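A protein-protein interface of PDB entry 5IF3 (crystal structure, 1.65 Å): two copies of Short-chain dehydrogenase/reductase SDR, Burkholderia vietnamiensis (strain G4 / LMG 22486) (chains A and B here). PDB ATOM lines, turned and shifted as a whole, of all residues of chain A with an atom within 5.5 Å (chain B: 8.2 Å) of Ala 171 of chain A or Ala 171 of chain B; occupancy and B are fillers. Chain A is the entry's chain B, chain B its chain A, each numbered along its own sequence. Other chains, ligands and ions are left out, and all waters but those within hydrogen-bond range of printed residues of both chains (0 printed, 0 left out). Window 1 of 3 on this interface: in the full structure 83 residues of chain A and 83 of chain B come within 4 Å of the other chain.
The backbone carbonyl oxygen (O) of Ala 155 of chain B sits at hydrogen-bond distance from a ring nitrogen (NE2) of His 175 of chain A (2.8 Å). The backbone carbonyl oxygen (O) of Ala 156 of chain B is in hydrogen-bond range of a ring nitrogen (NE2) of His 175 of chain A, 3.4 Å away. A ring nitrogen (NE2) of His 175 of chain A is in hydrogen-bond range of the backbone carbonyl oxygen of Asn 158 of chain B. O of Ala 155 of chain A sits at hydrogen-bond distance from NE2 of His 175 of chain B (2.9 Å). A ring nitrogen (NE2) of His 175 of chain B sits at hydrogen-bond distance from the backbone carbonyl oxygen (O) of Ala 156 of chain A.
Printed residues of chain B within 4 Å of Ala 156 of chain A: His 175. Ala 171 of chain A touches two residues of chain B. Printed residues of chain A within 4 Å of Ala 155 of chain B: His 175. Of the printed residues of chain A, Cys 167 of chain B touches His 175 (3.3 Å). Of the printed residues of chain A, Ala 168 of chain B touches Ala 172 (3.2 Å) and His 176 (3.8 Å). Ala 171 of chain B touches two residues of chain A. Printed residues of chain A within 4 Å of His 176 of chain B: Ala 168. The nearest residue of chain B that does not touch Ala 171 of chain A is Ala 172 of chain B (4.6 Å).
Hydrophobic or aromatic side chains of chain A within 4 Å of the printed part of chain B: Ala 168, Ala 171, Ala 172, His 175 and His 176. Of the 27 printed residues of chain B, 12 touch a printed residue of chain A. Printed residues of chain B that touch a printed residue of chain A: Ala 155, Ala 156, Arg 157, Asn 158, Ser 164, Cys 167, Ala 168, Ala 171, Ala 172, His 175, His 176 and Thr 253. Hydrophobic or aromatic side chains of chain B within 4 Å of the printed part of chain A: Ala 168, Ala 171, Ala 172, His 175 and His 176. Along chain B the printed residues that touch a printed residue of chain A span positions 155 to 253. Among the printed residues, 17 pairs touch across the chains.
The backbone carbonyl oxygen (O) of Gly 154 of chain B lies within hydrogen-bond range of the side-chain amide nitrogen (ND2) of Asn 158 of chain B, 3.1 Å away. NH2 of Arg 157 of chain B lies within hydrogen-bond range of O of Ser 192 of chain B (3.0 Å). The guanidinium group (NH1) of Arg 178 of chain B lies within hydrogen-bond range of a ring nitrogen (ND1) of His 175 of chain B. SG of Cys 167 of chain A lies close to O of Ala 155 of chain A (3.5 Å).
Ala 155 of chain A touches His 175 of chain B, and with the chains exchanged His 175 of chain A touches Ala 155 of chain B. Ala 156 of chain A touches His 175 of chain B, and with the chains exchanged His 175 of chain A touches Ala 156 of chain B. Ala 168 of chain A touches Ala 172 of chain B, and with the chains exchanged Ala 172 of chain A touches Ala 168 of chain B. Ala 171 of chain A touches its own counterpart, Ala 171 of chain B. Positions printed for both chains: 155, 156, 166, 167, 168, 169, 170, 171, 172, 173, 174, 175, 176 and 178.
CB of Ala 172 of chain B touches O of Ala 168 of chain A, 3.3 Å away. Ala 168 of chain A touches His 176 of chain B. Ala 171 of chain A touches Ala 171 of chain B. Ala 171 of chain A touches His 175 of chain B (CB to CB, 3.5 Å). O of Ala 168 of chain B touches CB of Ala 172 of chain A, 3.2 Å away. His 175 of chain A touches Cys 167 of chain B (CD2 to O, 3.3 Å). CB of Ala 171 of chain B touches CB of His 175 of chain A (3.5 Å). His 176 of chain A touches Ala 168 of chain B (CB to CB, 3.8 Å).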
ATOM      1  N   ALA A 155       4.388 -17.354   8.881  1.00  0.00           N
ATOM      2  CA  ALA A 155       5.680 -16.692   8.751  1.00  0.00           C
ATOM      3  C   ALA A 155       5.743 -15.710   7.583  1.00  0.00           C
ATOM      4  O   ALA A 155       6.705 -14.941   7.505  1.00  0.00           O
ATOM      5  CB  ALA A 155       6.777 -17.749   8.603  1.00  0.00           C
ATOM      6  N   ALA A 156       4.776 -15.726   6.661  1.00  0.00           N
ATOM      7  CA  ALA A 156       4.715 -14.687   5.630  1.00  0.00           C
ATOM      8  C   ALA A 156       4.317 -13.338   6.202  1.00  0.00           C
ATOM      9  O   ALA A 156       4.600 -12.300   5.584  1.00  0.00           O
ATOM     10  CB  ALA A 156       3.712 -15.064   4.535  1.00  0.00           C
ATOM     11  N   TYR A 166      12.970 -18.128   5.042  1.00  0.00           N
ATOM     12  CA  TYR A 166      11.626 -18.644   4.833  1.00  0.00           C
ATOM     13  C   TYR A 166      10.597 -17.523   4.907  1.00  0.00           C
ATOM     14  O   TYR A 166       9.713 -17.420   4.046  1.00  0.00           O
ATOM     15  CB  TYR A 166      11.325 -19.727   5.872  1.00  0.00           C
ATOM     16  CG  TYR A 166      10.026 -20.463   5.642  1.00  0.00           C
ATOM     17  CD1 TYR A 166       9.906 -21.391   4.616  1.00  0.00           C
ATOM     18  CD2 TYR A 166       8.943 -20.258   6.480  1.00  0.00           C
ATOM     19  CE1 TYR A 166       8.741 -22.104   4.427  1.00  0.00           C
ATOM     20  CE2 TYR A 166       7.767 -20.956   6.288  1.00  0.00           C
ATOM     21  CZ  TYR A 166       7.672 -21.870   5.261  1.00  0.00           C
ATOM     22  OH  TYR A 166       6.508 -22.570   5.073  1.00  0.00           O
ATOM     23  N   CYS A 167      10.705 -16.669   5.933  1.00  0.00           N
ATOM     24  CA  CYS A 167       9.826 -15.507   6.072  1.00  0.00           C
ATOM     25  C   CYS A 167       9.816 -14.663   4.804  1.00  0.00           C
ATOM     26  O   CYS A 167       8.749 -14.300   4.286  1.00  0.00           O
ATOM     27  CB  CYS A 167      10.268 -14.651   7.263  1.00  0.00           C
ATOM     28  SG  CYS A 167       9.889 -15.360   8.901  1.00  0.00           S
ATOM     29  N   ALA A 168      11.004 -14.309   4.307  1.00  0.00           N
ATOM     30  CA  ALA A 168      11.087 -13.501   3.094  1.00  0.00           C
ATOM     31  C   ALA A 168      10.365 -14.173   1.933  1.00  0.00           C
ATOM     32  O   ALA A 168       9.609 -13.517   1.204  1.00  0.00           O
ATOM     33  CB  ALA A 168      12.563 -13.253   2.741  1.00  0.00           C
ATOM     34  N   THR A 169      10.581 -15.479   1.748  1.00  0.00           N
ATOM     35  CA  THR A 169      10.019 -16.157   0.578  1.00  0.00           C
ATOM     36  C   THR A 169       8.495 -16.221   0.634  1.00  0.00           C
ATOM     37  O   THR A 169       7.827 -16.069  -0.399  1.00  0.00           O
ATOM     38  CB  THR A 169      10.602 -17.569   0.414  1.00  0.00           C
ATOM     39  OG1 THR A 169      10.189 -18.429   1.485  1.00  0.00           O
ATOM     40  CG2 THR A 169      12.122 -17.529   0.349  1.00  0.00           C
ATOM     41  N   LYS A 170       7.923 -16.447   1.818  1.00  0.00           N
ATOM     42  CA  LYS A 170       6.471 -16.560   1.889  1.00  0.00           C
ATOM     43  C   LYS A 170       5.812 -15.194   1.829  1.00  0.00           C
ATOM     44  O   LYS A 170       4.726 -15.060   1.254  1.00  0.00           O
ATOM     45  CB  LYS A 170       6.060 -17.328   3.147  1.00  0.00           C
ATOM     46  CG  LYS A 170       6.503 -18.818   3.136  1.00  0.00           C
ATOM     47  CD  LYS A 170       6.030 -19.538   1.870  1.00  0.00           C
ATOM     48  CE  LYS A 170       6.262 -21.050   1.975  1.00  0.00           C
ATOM     49  NZ  LYS A 170       5.687 -21.800   0.824  1.00  0.00           N
ATOM     50  N   ALA A 171       6.481 -14.157   2.347  1.00  0.00           N
ATOM     51  CA  ALA A 171       5.956 -12.807   2.175  1.00  0.00           C
ATOM     52  C   ALA A 171       5.859 -12.438   0.699  1.00  0.00           C
ATOM     53  O   ALA A 171       4.934 -11.718   0.299  1.00  0.00           O
ATOM     54  CB  ALA A 171       6.847 -11.799   2.913  1.00  0.00           C
ATOM     55  N   ALA A 172       6.797 -12.924  -0.118  1.00  0.00           N
ATOM     56  CA  ALA A 172       6.740 -12.661  -1.554  1.00  0.00           C
ATOM     57  C   ALA A 172       5.497 -13.280  -2.185  1.00  0.00           C
ATOM     58  O   ALA A 172       4.862 -12.667  -3.056  1.00  0.00           O
ATOM     59  CB  ALA A 172       8.007 -13.197  -2.223  1.00  0.00           C
ATOM     60  N   LEU A 173       5.145 -14.500  -1.769  1.00  0.00           N
ATOM     61  CA  LEU A 173       3.947 -15.147  -2.305  1.00  0.00           C
ATOM     62  C   LEU A 173       2.688 -14.362  -1.956  1.00  0.00           C
ATOM     63  O   LEU A 173       1.800 -14.206  -2.802  1.00  0.00           O
ATOM     64  CB  LEU A 173       3.835 -16.585  -1.794  1.00  0.00           C
ATOM     65  CG  LEU A 173       4.982 -17.523  -2.218  1.00  0.00           C
ATOM     66  CD1 LEU A 173       4.658 -18.973  -1.842  1.00  0.00           C
ATOM     67  CD2 LEU A 173       5.260 -17.407  -3.718  1.00  0.00           C
ATOM     68  N   ASP A 174       2.586 -13.863  -0.717  1.00  0.00           N
ATOM     69  CA  ASP A 174       1.414 -13.066  -0.341  1.00  0.00           C
ATOM     70  C   ASP A 174       1.268 -11.852  -1.253  1.00  0.00           C
ATOM     71  O   ASP A 174       0.177 -11.561  -1.756  1.00  0.00           O
ATOM     72  CB  ASP A 174       1.522 -12.574   1.104  1.00  0.00           C
ATOM     73  CG  ASP A 174       1.161 -13.627   2.155  1.00  0.00           C
ATOM     74  OD1 ASP A 174       0.843 -14.795   1.824  1.00  0.00           O
ATOM     75  OD2 ASP A 174       1.194 -13.246   3.344  1.00  0.00           O
ATOM     76  N   HIS A 175       2.360 -11.112  -1.458  1.00  0.00           N
ATOM     77  CA  HIS A 175       2.214  -9.858  -2.182  1.00  0.00           C
ATOM     78  C   HIS A 175       2.047 -10.090  -3.677  1.00  0.00           C
ATOM     79  O   HIS A 175       1.388  -9.294  -4.355  1.00  0.00           O
ATOM     80  CB  HIS A 175       3.406  -8.945  -1.886  1.00  0.00           C
ATOM     81  CG  HIS A 175       3.052  -7.495  -1.919  1.00  0.00           C
ATOM     82  ND1 HIS A 175       1.849  -7.011  -1.435  1.00  0.00           N
ATOM     83  CD2 HIS A 175       3.726  -6.425  -2.400  1.00  0.00           C
ATOM     84  CE1 HIS A 175       1.811  -5.702  -1.611  1.00  0.00           C
ATOM     85  NE2 HIS A 175       2.940  -5.320  -2.188  1.00  0.00           N
ATOM     86  N   HIS A 176       2.631 -11.174  -4.201  1.00  0.00           N
ATOM     87  CA  HIS A 176       2.347 -11.598  -5.566  1.00  0.00           C
ATOM     88  C   HIS A 176       0.847 -11.762  -5.774  1.00  0.00           C
ATOM     89  O   HIS A 176       0.272 -11.222  -6.726  1.00  0.00           O
ATOM     90  CB  HIS A 176       3.070 -12.913  -5.848  1.00  0.00           C
ATOM     91  CG  HIS A 176       2.909 -13.414  -7.248  1.00  0.00           C
ATOM     92  ND1 HIS A 176       2.158 -14.527  -7.556  1.00  0.00           N
ATOM     93  CD2 HIS A 176       3.437 -12.981  -8.416  1.00  0.00           C
ATOM     94  CE1 HIS A 176       2.212 -14.746  -8.858  1.00  0.00           C
ATOM     95  NE2 HIS A 176       2.983 -13.821  -9.403  1.00  0.00           N
ATOM     96  N   ARG A 178      -1.628 -10.489  -4.040  1.00  0.00           N
ATOM     97  CA  ARG A 178      -2.326  -9.210  -3.946  1.00  0.00           C
ATOM     98  C   ARG A 178      -2.279  -8.451  -5.263  1.00  0.00           C
ATOM     99  O   ARG A 178      -3.280  -7.867  -5.690  1.00  0.00           O
ATOM    100  CB  ARG A 178      -1.734  -8.345  -2.837  1.00  0.00           C
ATOM    101  CG  ARG A 178      -1.901  -8.907  -1.435  1.00  0.00           C
ATOM    102  CD  ARG A 178      -1.451  -7.885  -0.400  1.00  0.00           C
ATOM    103  NE  ARG A 178      -1.379  -8.489   0.918  1.00  0.00           N
ATOM    104  CZ  ARG A 178      -0.262  -8.926   1.487  1.00  0.00           C
ATOM    105  NH1 ARG A 178       0.922  -8.799   0.878  1.00  0.00           N
ATOM    106  NH2 ARG A 178      -0.328  -9.482   2.686  1.00  0.00           N
ATOM    107  N   ASN B 125      16.538  -9.637  -7.593  1.00  0.00           N
ATOM    108  CA  ASN B 125      15.880  -8.764  -6.624  1.00  0.00           C
ATOM    109  C   ASN B 125      15.805  -9.376  -5.231  1.00  0.00           C
ATOM    110  O   ASN B 125      15.695  -8.626  -4.253  1.00  0.00           O
ATOM    111  CB  ASN B 125      14.449  -8.445  -7.043  1.00  0.00           C
ATOM    112  CG  ASN B 125      14.356  -7.568  -8.269  1.00  0.00           C
ATOM    113  OD1 ASN B 125      15.339  -7.302  -8.958  1.00  0.00           O
ATOM    114  ND2 ASN B 125      13.140  -7.121  -8.556  1.00  0.00           N
ATOM    115  N   VAL B 126      15.816 -10.711  -5.126  1.00  0.00           N
ATOM    116  CA  VAL B 126      15.628 -11.388  -3.838  1.00  0.00           C
ATOM    117  C   VAL B 126      16.854 -12.215  -3.484  1.00  0.00           C
ATOM    118  O   VAL B 126      17.415 -12.072  -2.392  1.00  0.00           O
ATOM    119  CB  VAL B 126      14.382 -12.289  -3.814  1.00  0.00           C
ATOM    120  CG1 VAL B 126      14.216 -12.897  -2.423  1.00  0.00           C
ATOM    121  CG2 VAL B 126      13.139 -11.492  -4.170  1.00  0.00           C
ATOM    122  N   HIS B 150      18.428  -2.701   2.542  1.00  0.00           N
ATOM    123  CA  HIS B 150      17.758  -3.158   1.337  1.00  0.00           C
ATOM    124  C   HIS B 150      17.059  -1.961   0.714  1.00  0.00           C
ATOM    125  O   HIS B 150      16.288  -1.276   1.393  1.00  0.00           O
ATOM    126  CB  HIS B 150      16.696  -4.227   1.634  1.00  0.00           C
ATOM    127  CG  HIS B 150      17.215  -5.522   2.183  1.00  0.00           C
ATOM    128  ND1 HIS B 150      18.452  -6.061   1.863  1.00  0.00           N
ATOM    129  CD2 HIS B 150      16.613  -6.416   3.000  1.00  0.00           C
ATOM    130  CE1 HIS B 150      18.586  -7.223   2.483  1.00  0.00           C
ATOM    131  NE2 HIS B 150      17.485  -7.459   3.187  1.00  0.00           N
ATOM    132  N   SER B 152      14.127  -0.847  -0.950  1.00  0.00           N
ATOM    133  CA  SER B 152      12.812  -1.441  -1.136  1.00  0.00           C
ATOM    134  C   SER B 152      11.978  -0.555  -2.053  1.00  0.00           C
ATOM    135  O   SER B 152      12.518   0.072  -2.977  1.00  0.00           O
ATOM    136  CB  SER B 152      12.141  -1.667   0.223  1.00  0.00           C
ATOM    137  OG  SER B 152      10.915  -2.382   0.076  1.00  0.00           O
ATOM    138  N   SER B 153      10.671  -0.483  -1.812  1.00  0.00           N
ATOM    139  CA  SER B 153       9.782   0.266  -2.687  1.00  0.00           C
ATOM    140  C   SER B 153       8.446   0.421  -1.986  1.00  0.00           C
ATOM    141  O   SER B 153       8.088  -0.402  -1.137  1.00  0.00           O
ATOM    142  CB  SER B 153       9.580  -0.445  -4.033  1.00  0.00           C
ATOM    143  OG  SER B 153       8.629   0.245  -4.838  1.00  0.00           O
ATOM    144  N   GLY B 154       7.718   1.472  -2.349  1.00  0.00           N
ATOM    145  CA  GLY B 154       6.312   1.515  -1.997  1.00  0.00           C
ATOM    146  C   GLY B 154       5.580   0.274  -2.461  1.00  0.00           C
ATOM    147  O   GLY B 154       4.627  -0.170  -1.812  1.00  0.00           O
ATOM    148  N   ALA B 155       6.040  -0.329  -3.566  1.00  0.00           N
ATOM    149  CA  ALA B 155       5.446  -1.559  -4.081  1.00  0.00           C
ATOM    150  C   ALA B 155       5.659  -2.764  -3.171  1.00  0.00           C
ATOM    151  O   ALA B 155       5.016  -3.798  -3.397  1.00  0.00           O
ATOM    152  CB  ALA B 155       6.004  -1.882  -5.466  1.00  0.00           C
ATOM    153  N   ALA B 156       6.543  -2.676  -2.173  1.00  0.00           N
ATOM    154  CA  ALA B 156       6.684  -3.763  -1.207  1.00  0.00           C
ATOM    155  C   ALA B 156       5.500  -3.818  -0.252  1.00  0.00           C
ATOM    156  O   ALA B 156       5.222  -4.877   0.343  1.00  0.00           O
ATOM    157  CB  ALA B 156       7.980  -3.594  -0.413  1.00  0.00           C
ATOM    158  N   ARG B 157       4.795  -2.703  -0.105  1.00  0.00           N
ATOM    159  CA  ARG B 157       3.757  -2.528   0.896  1.00  0.00           C
ATOM    160  C   ARG B 157       2.386  -2.307   0.291  1.00  0.00           C
ATOM    161  O   ARG B 157       1.379  -2.631   0.928  1.00  0.00           O
ATOM    162  CB  ARG B 157       4.109  -1.337   1.809  1.00  0.00           C
ATOM    163  CG  ARG B 157       5.434  -1.541   2.550  1.00  0.00           C
ATOM    164  CD  ARG B 157       6.497  -0.507   2.183  1.00  0.00           C
ATOM    165  NE  ARG B 157       7.834  -0.950   2.592  1.00  0.00           N
ATOM    166  CZ  ARG B 157       8.829  -0.133   2.945  1.00  0.00           C
ATOM    167  NH1 ARG B 157       8.635   1.193   2.952  1.00  0.00           N
ATOM    168  NH2 ARG B 157      10.008  -0.654   3.301  1.00  0.00           N
ATOM    169  N   ASN B 158       2.325  -1.763  -0.918  1.00  0.00           N
ATOM    170  CA  ASN B 158       1.083  -1.613  -1.658  1.00  0.00           C
ATOM    171  C   ASN B 158       1.189  -2.440  -2.929  1.00  0.00           C
ATOM    172  O   ASN B 158       2.251  -2.491  -3.549  1.00  0.00           O
ATOM    173  CB  ASN B 158       0.825  -0.141  -1.995  1.00  0.00           C
ATOM    174  CG  ASN B 158       1.013   0.772  -0.797  1.00  0.00           C
ATOM    175  OD1 ASN B 158       0.118   0.914   0.034  1.00  0.00           O
ATOM    176  ND2 ASN B 158       2.190   1.390  -0.697  1.00  0.00           N
ATOM    177  N   SER B 164       3.166  -7.495 -10.346  1.00  0.00           N
ATOM    178  CA  SER B 164       3.123  -8.581  -9.367  1.00  0.00           C
ATOM    179  C   SER B 164       4.513  -9.139  -9.067  1.00  0.00           C
ATOM    180  O   SER B 164       4.804  -9.505  -7.921  1.00  0.00           O
ATOM    181  CB  SER B 164       2.184  -9.693  -9.837  1.00  0.00           C
ATOM    182  OG  SER B 164       2.500 -10.138 -11.141  1.00  0.00           O
ATOM    183  N   VAL B 165       5.383  -9.218 -10.074  1.00  0.00           N
ATOM    184  CA  VAL B 165       6.721  -9.757  -9.828  1.00  0.00           C
ATOM    185  C   VAL B 165       7.535  -8.797  -8.967  1.00  0.00           C
ATOM    186  O   VAL B 165       8.107  -9.192  -7.946  1.00  0.00           O
ATOM    187  CB  VAL B 165       7.440 -10.076 -11.151  1.00  0.00           C
ATOM    188  CG1 VAL B 165       8.887 -10.510 -10.874  1.00  0.00           C
ATOM    189  CG2 VAL B 165       6.691 -11.161 -11.913  1.00  0.00           C
ATOM    190  N   TYR B 166       7.603  -7.520  -9.365  1.00  0.00           N
ATOM    191  CA  TYR B 166       8.341  -6.535  -8.578  1.00  0.00           C
ATOM    192  C   TYR B 166       7.797  -6.444  -7.159  1.00  0.00           C
ATOM    193  O   TYR B 166       8.561  -6.442  -6.183  1.00  0.00           O
ATOM    194  CB  TYR B 166       8.262  -5.173  -9.264  1.00  0.00           C
ATOM    195  CG  TYR B 166       9.205  -4.144  -8.700  1.00  0.00           C
ATOM    196  CD1 TYR B 166      10.573  -4.243  -8.915  1.00  0.00           C
ATOM    197  CD2 TYR B 166       8.730  -3.061  -7.975  1.00  0.00           C
ATOM    198  CE1 TYR B 166      11.442  -3.286  -8.423  1.00  0.00           C
ATOM    199  CE2 TYR B 166       9.592  -2.097  -7.478  1.00  0.00           C
ATOM    200  CZ  TYR B 166      10.942  -2.212  -7.710  1.00  0.00           C
ATOM    201  OH  TYR B 166      11.800  -1.258  -7.214  1.00  0.00           O
ATOM    202  N   CYS B 167       6.474  -6.363  -7.028  1.00  0.00           N
ATOM    203  CA  CYS B 167       5.840  -6.314  -5.712  1.00  0.00           C
ATOM    204  C   CYS B 167       6.267  -7.497  -4.855  1.00  0.00           C
ATOM    205  O   CYS B 167       6.643  -7.335  -3.689  1.00  0.00           O
ATOM    206  CB  CYS B 167       4.319  -6.300  -5.867  1.00  0.00           C
ATOM    207  SG  CYS B 167       3.618  -4.719  -6.432  1.00  0.00           S
ATOM    208  N   ALA B 168       6.197  -8.703  -5.420  1.00  0.00           N
ATOM    209  CA  ALA B 168       6.603  -9.892  -4.678  1.00  0.00           C
ATOM    210  C   ALA B 168       8.043  -9.775  -4.190  1.00  0.00           C
ATOM    211  O   ALA B 168       8.343 -10.080  -3.028  1.00  0.00           O
ATOM    212  CB  ALA B 168       6.429 -11.135  -5.548  1.00  0.00           C
ATOM    213  N   THR B 169       8.955  -9.327  -5.064  1.00  0.00           N
ATOM    214  CA  THR B 169      10.364  -9.320  -4.682  1.00  0.00           C
ATOM    215  C   THR B 169      10.653  -8.293  -3.597  1.00  0.00           C
ATOM    216  O   THR B 169      11.467  -8.546  -2.706  1.00  0.00           O
ATOM    217  CB  THR B 169      11.273  -9.075  -5.891  1.00  0.00           C
ATOM    218  OG1 THR B 169      11.072  -7.762  -6.437  1.00  0.00           O
ATOM    219  CG2 THR B 169      11.052 -10.128  -6.952  1.00  0.00           C
ATOM    220  N   LYS B 170      10.016  -7.120  -3.655  1.00  0.00           N
ATOM    221  CA  LYS B 170      10.335  -6.122  -2.643  1.00  0.00           C
ATOM    222  C   LYS B 170       9.654  -6.440  -1.309  1.00  0.00           C
ATOM    223  O   LYS B 170      10.218  -6.151  -0.246  1.00  0.00           O
ATOM    224  CB  LYS B 170       9.968  -4.723  -3.163  1.00  0.00           C
ATOM    225  CG  LYS B 170      10.813  -4.273  -4.376  1.00  0.00           C
ATOM    226  CD  LYS B 170      12.311  -4.292  -4.043  1.00  0.00           C
ATOM    227  CE  LYS B 170      13.113  -3.523  -5.098  1.00  0.00           C
ATOM    228  NZ  LYS B 170      14.588  -3.514  -4.831  1.00  0.00           N
ATOM    229  N   ALA B 171       8.471  -7.063  -1.338  1.00  0.00           N
ATOM    230  CA  ALA B 171       7.872  -7.574  -0.103  1.00  0.00           C
ATOM    231  C   ALA B 171       8.801  -8.562   0.601  1.00  0.00           C
ATOM    232  O   ALA B 171       8.859  -8.597   1.837  1.00  0.00           O
ATOM    233  CB  ALA B 171       6.527  -8.225  -0.414  1.00  0.00           C
ATOM    234  N   ALA B 172       9.533  -9.372  -0.168  1.00  0.00           N
ATOM    235  CA  ALA B 172      10.483 -10.308   0.435  1.00  0.00           C
ATOM    236  C   ALA B 172      11.564  -9.575   1.219  1.00  0.00           C
ATOM    237  O   ALA B 172      11.941 -10.000   2.318  1.00  0.00           O
ATOM    238  CB  ALA B 172      11.117 -11.186  -0.650  1.00  0.00           C
ATOM    239  N   LEU B 173      12.097  -8.488   0.655  1.00  0.00           N
ATOM    240  CA  LEU B 173      13.162  -7.752   1.325  1.00  0.00           C
ATOM    241  C   LEU B 173      12.667  -7.142   2.631  1.00  0.00           C
ATOM    242  O   LEU B 173      13.376  -7.168   3.647  1.00  0.00           O
ATOM    243  CB  LEU B 173      13.723  -6.663   0.402  1.00  0.00           C
ATOM    244  CG  LEU B 173      14.334  -7.143  -0.921  1.00  0.00           C
ATOM    245  CD1 LEU B 173      14.958  -5.979  -1.691  1.00  0.00           C
ATOM    246  CD2 LEU B 173      15.388  -8.260  -0.687  1.00  0.00           C
ATOM    247  N   ASP B 174      11.438  -6.609   2.637  1.00  0.00           N
ATOM    248  CA  ASP B 174      10.896  -6.053   3.871  1.00  0.00           C
ATOM    249  C   ASP B 174      10.849  -7.115   4.961  1.00  0.00           C
ATOM    250  O   ASP B 174      11.223  -6.863   6.110  1.00  0.00           O
ATOM    251  CB  ASP B 174       9.475  -5.515   3.659  1.00  0.00           C
ATOM    252  CG  ASP B 174       9.422  -4.140   3.026  1.00  0.00           C
ATOM    253  OD1 ASP B 174      10.461  -3.573   2.631  1.00  0.00           O
ATOM    254  OD2 ASP B 174       8.272  -3.637   2.908  1.00  0.00           O
ATOM    255  N   HIS B 175      10.337  -8.298   4.627  1.00  0.00           N
ATOM    256  CA  HIS B 175      10.123  -9.290   5.679  1.00  0.00           C
ATOM    257  C   HIS B 175      11.426  -9.953   6.089  1.00  0.00           C
ATOM    258  O   HIS B 175      11.575 -10.350   7.246  1.00  0.00           O
ATOM    259  CB  HIS B 175       9.092 -10.328   5.229  1.00  0.00           C
ATOM    260  CG  HIS B 175       8.300 -10.899   6.363  1.00  0.00           C
ATOM    261  ND1 HIS B 175       7.846 -10.121   7.407  1.00  0.00           N
ATOM    262  CD2 HIS B 175       7.906 -12.168   6.632  1.00  0.00           C
ATOM    263  CE1 HIS B 175       7.187 -10.886   8.265  1.00  0.00           C
ATOM    264  NE2 HIS B 175       7.215 -12.133   7.822  1.00  0.00           N
ATOM    265  N   HIS B 176      12.389 -10.047   5.171  1.00  0.00           N
ATOM    266  CA  HIS B 176      13.730 -10.476   5.542  1.00  0.00           C
ATOM    267  C   HIS B 176      14.282  -9.596   6.655  1.00  0.00           C
ATOM    268  O   HIS B 176      14.760 -10.089   7.686  1.00  0.00           O
ATOM    269  CB  HIS B 176      14.614 -10.422   4.297  1.00  0.00           C
ATOM    270  CG  HIS B 176      16.008 -10.932   4.510  1.00  0.00           C
ATOM    271  ND1 HIS B 176      17.111 -10.105   4.469  1.00  0.00           N
ATOM    272  CD2 HIS B 176      16.481 -12.180   4.759  1.00  0.00           C
ATOM    273  CE1 HIS B 176      18.207 -10.823   4.663  1.00  0.00           C
ATOM    274  NE2 HIS B 176      17.853 -12.084   4.841  1.00  0.00           N
ATOM    275  N   ALA B 177      14.187  -8.274   6.473  1.00  0.00           N
ATOM    276  CA  ALA B 177      14.693  -7.349   7.478  1.00  0.00           C
ATOM    277  C   ALA B 177      13.981  -7.523   8.812  1.00  0.00           C
ATOM    278  O   ALA B 177      14.623  -7.486   9.866  1.00  0.00           O
ATOM    279  CB  ALA B 177      14.559  -5.904   6.981  1.00  0.00           C
ATOM    280  N   ARG B 178      12.650  -7.693   8.793  1.00  0.00           N
ATOM    281  CA  ARG B 178      11.916  -7.855  10.046  1.00  0.00           C
ATOM    282  C   ARG B 178      12.435  -9.052  10.828  1.00  0.00           C
ATOM    283  O   ARG B 178      12.582  -8.984  12.051  1.00  0.00           O
ATOM    284  CB  ARG B 178      10.411  -8.013   9.786  1.00  0.00           C
ATOM    285  CG  ARG B 178       9.736  -6.772   9.190  1.00  0.00           C
ATOM    286  CD  ARG B 178       8.203  -6.940   9.121  1.00  0.00           C
ATOM    287  NE  ARG B 178       7.612  -5.902   8.281  1.00  0.00           N
ATOM    288  CZ  ARG B 178       7.270  -6.079   7.010  1.00  0.00           C
ATOM    289  NH1 ARG B 178       7.393  -7.270   6.439  1.00  0.00           N
ATOM    290  NH2 ARG B 178       6.776  -5.065   6.321  1.00  0.00           N
ATOM    291  N   SER B 192      14.951  -2.231   5.591  1.00  0.00           N
ATOM    292  CA  SER B 192      14.474  -2.248   4.210  1.00  0.00           C
ATOM    293  C   SER B 192      13.793  -0.906   3.950  1.00  0.00           C
ATOM    294  O   SER B 192      12.740  -0.613   4.533  1.00  0.00           O
ATOM    295  CB  SER B 192      13.527  -3.430   3.997  1.00  0.00           C
ATOM    296  OG  SER B 192      13.157  -3.565   2.630  1.00  0.00           O
ATOM    297  N   THR B 253      -5.227 -13.121   0.253  1.00  0.00           N
ATOM    298  CA  THR B 253      -4.538 -13.940   1.242  1.00  0.00           C
ATOM    299  C   THR B 253      -5.566 -14.537   2.192  1.00  0.00           C
ATOM    300  O   THR B 253      -6.677 -14.023   2.331  1.00  0.00           O
ATOM    301  CB  THR B 253      -3.510 -13.137   2.050  1.00  0.00           C
ATOM    302  OG1 THR B 253      -4.177 -12.139   2.823  1.00  0.00           O
ATOM    303  CG2 THR B 253      -2.482 -12.475   1.134  1.00  0.00           C
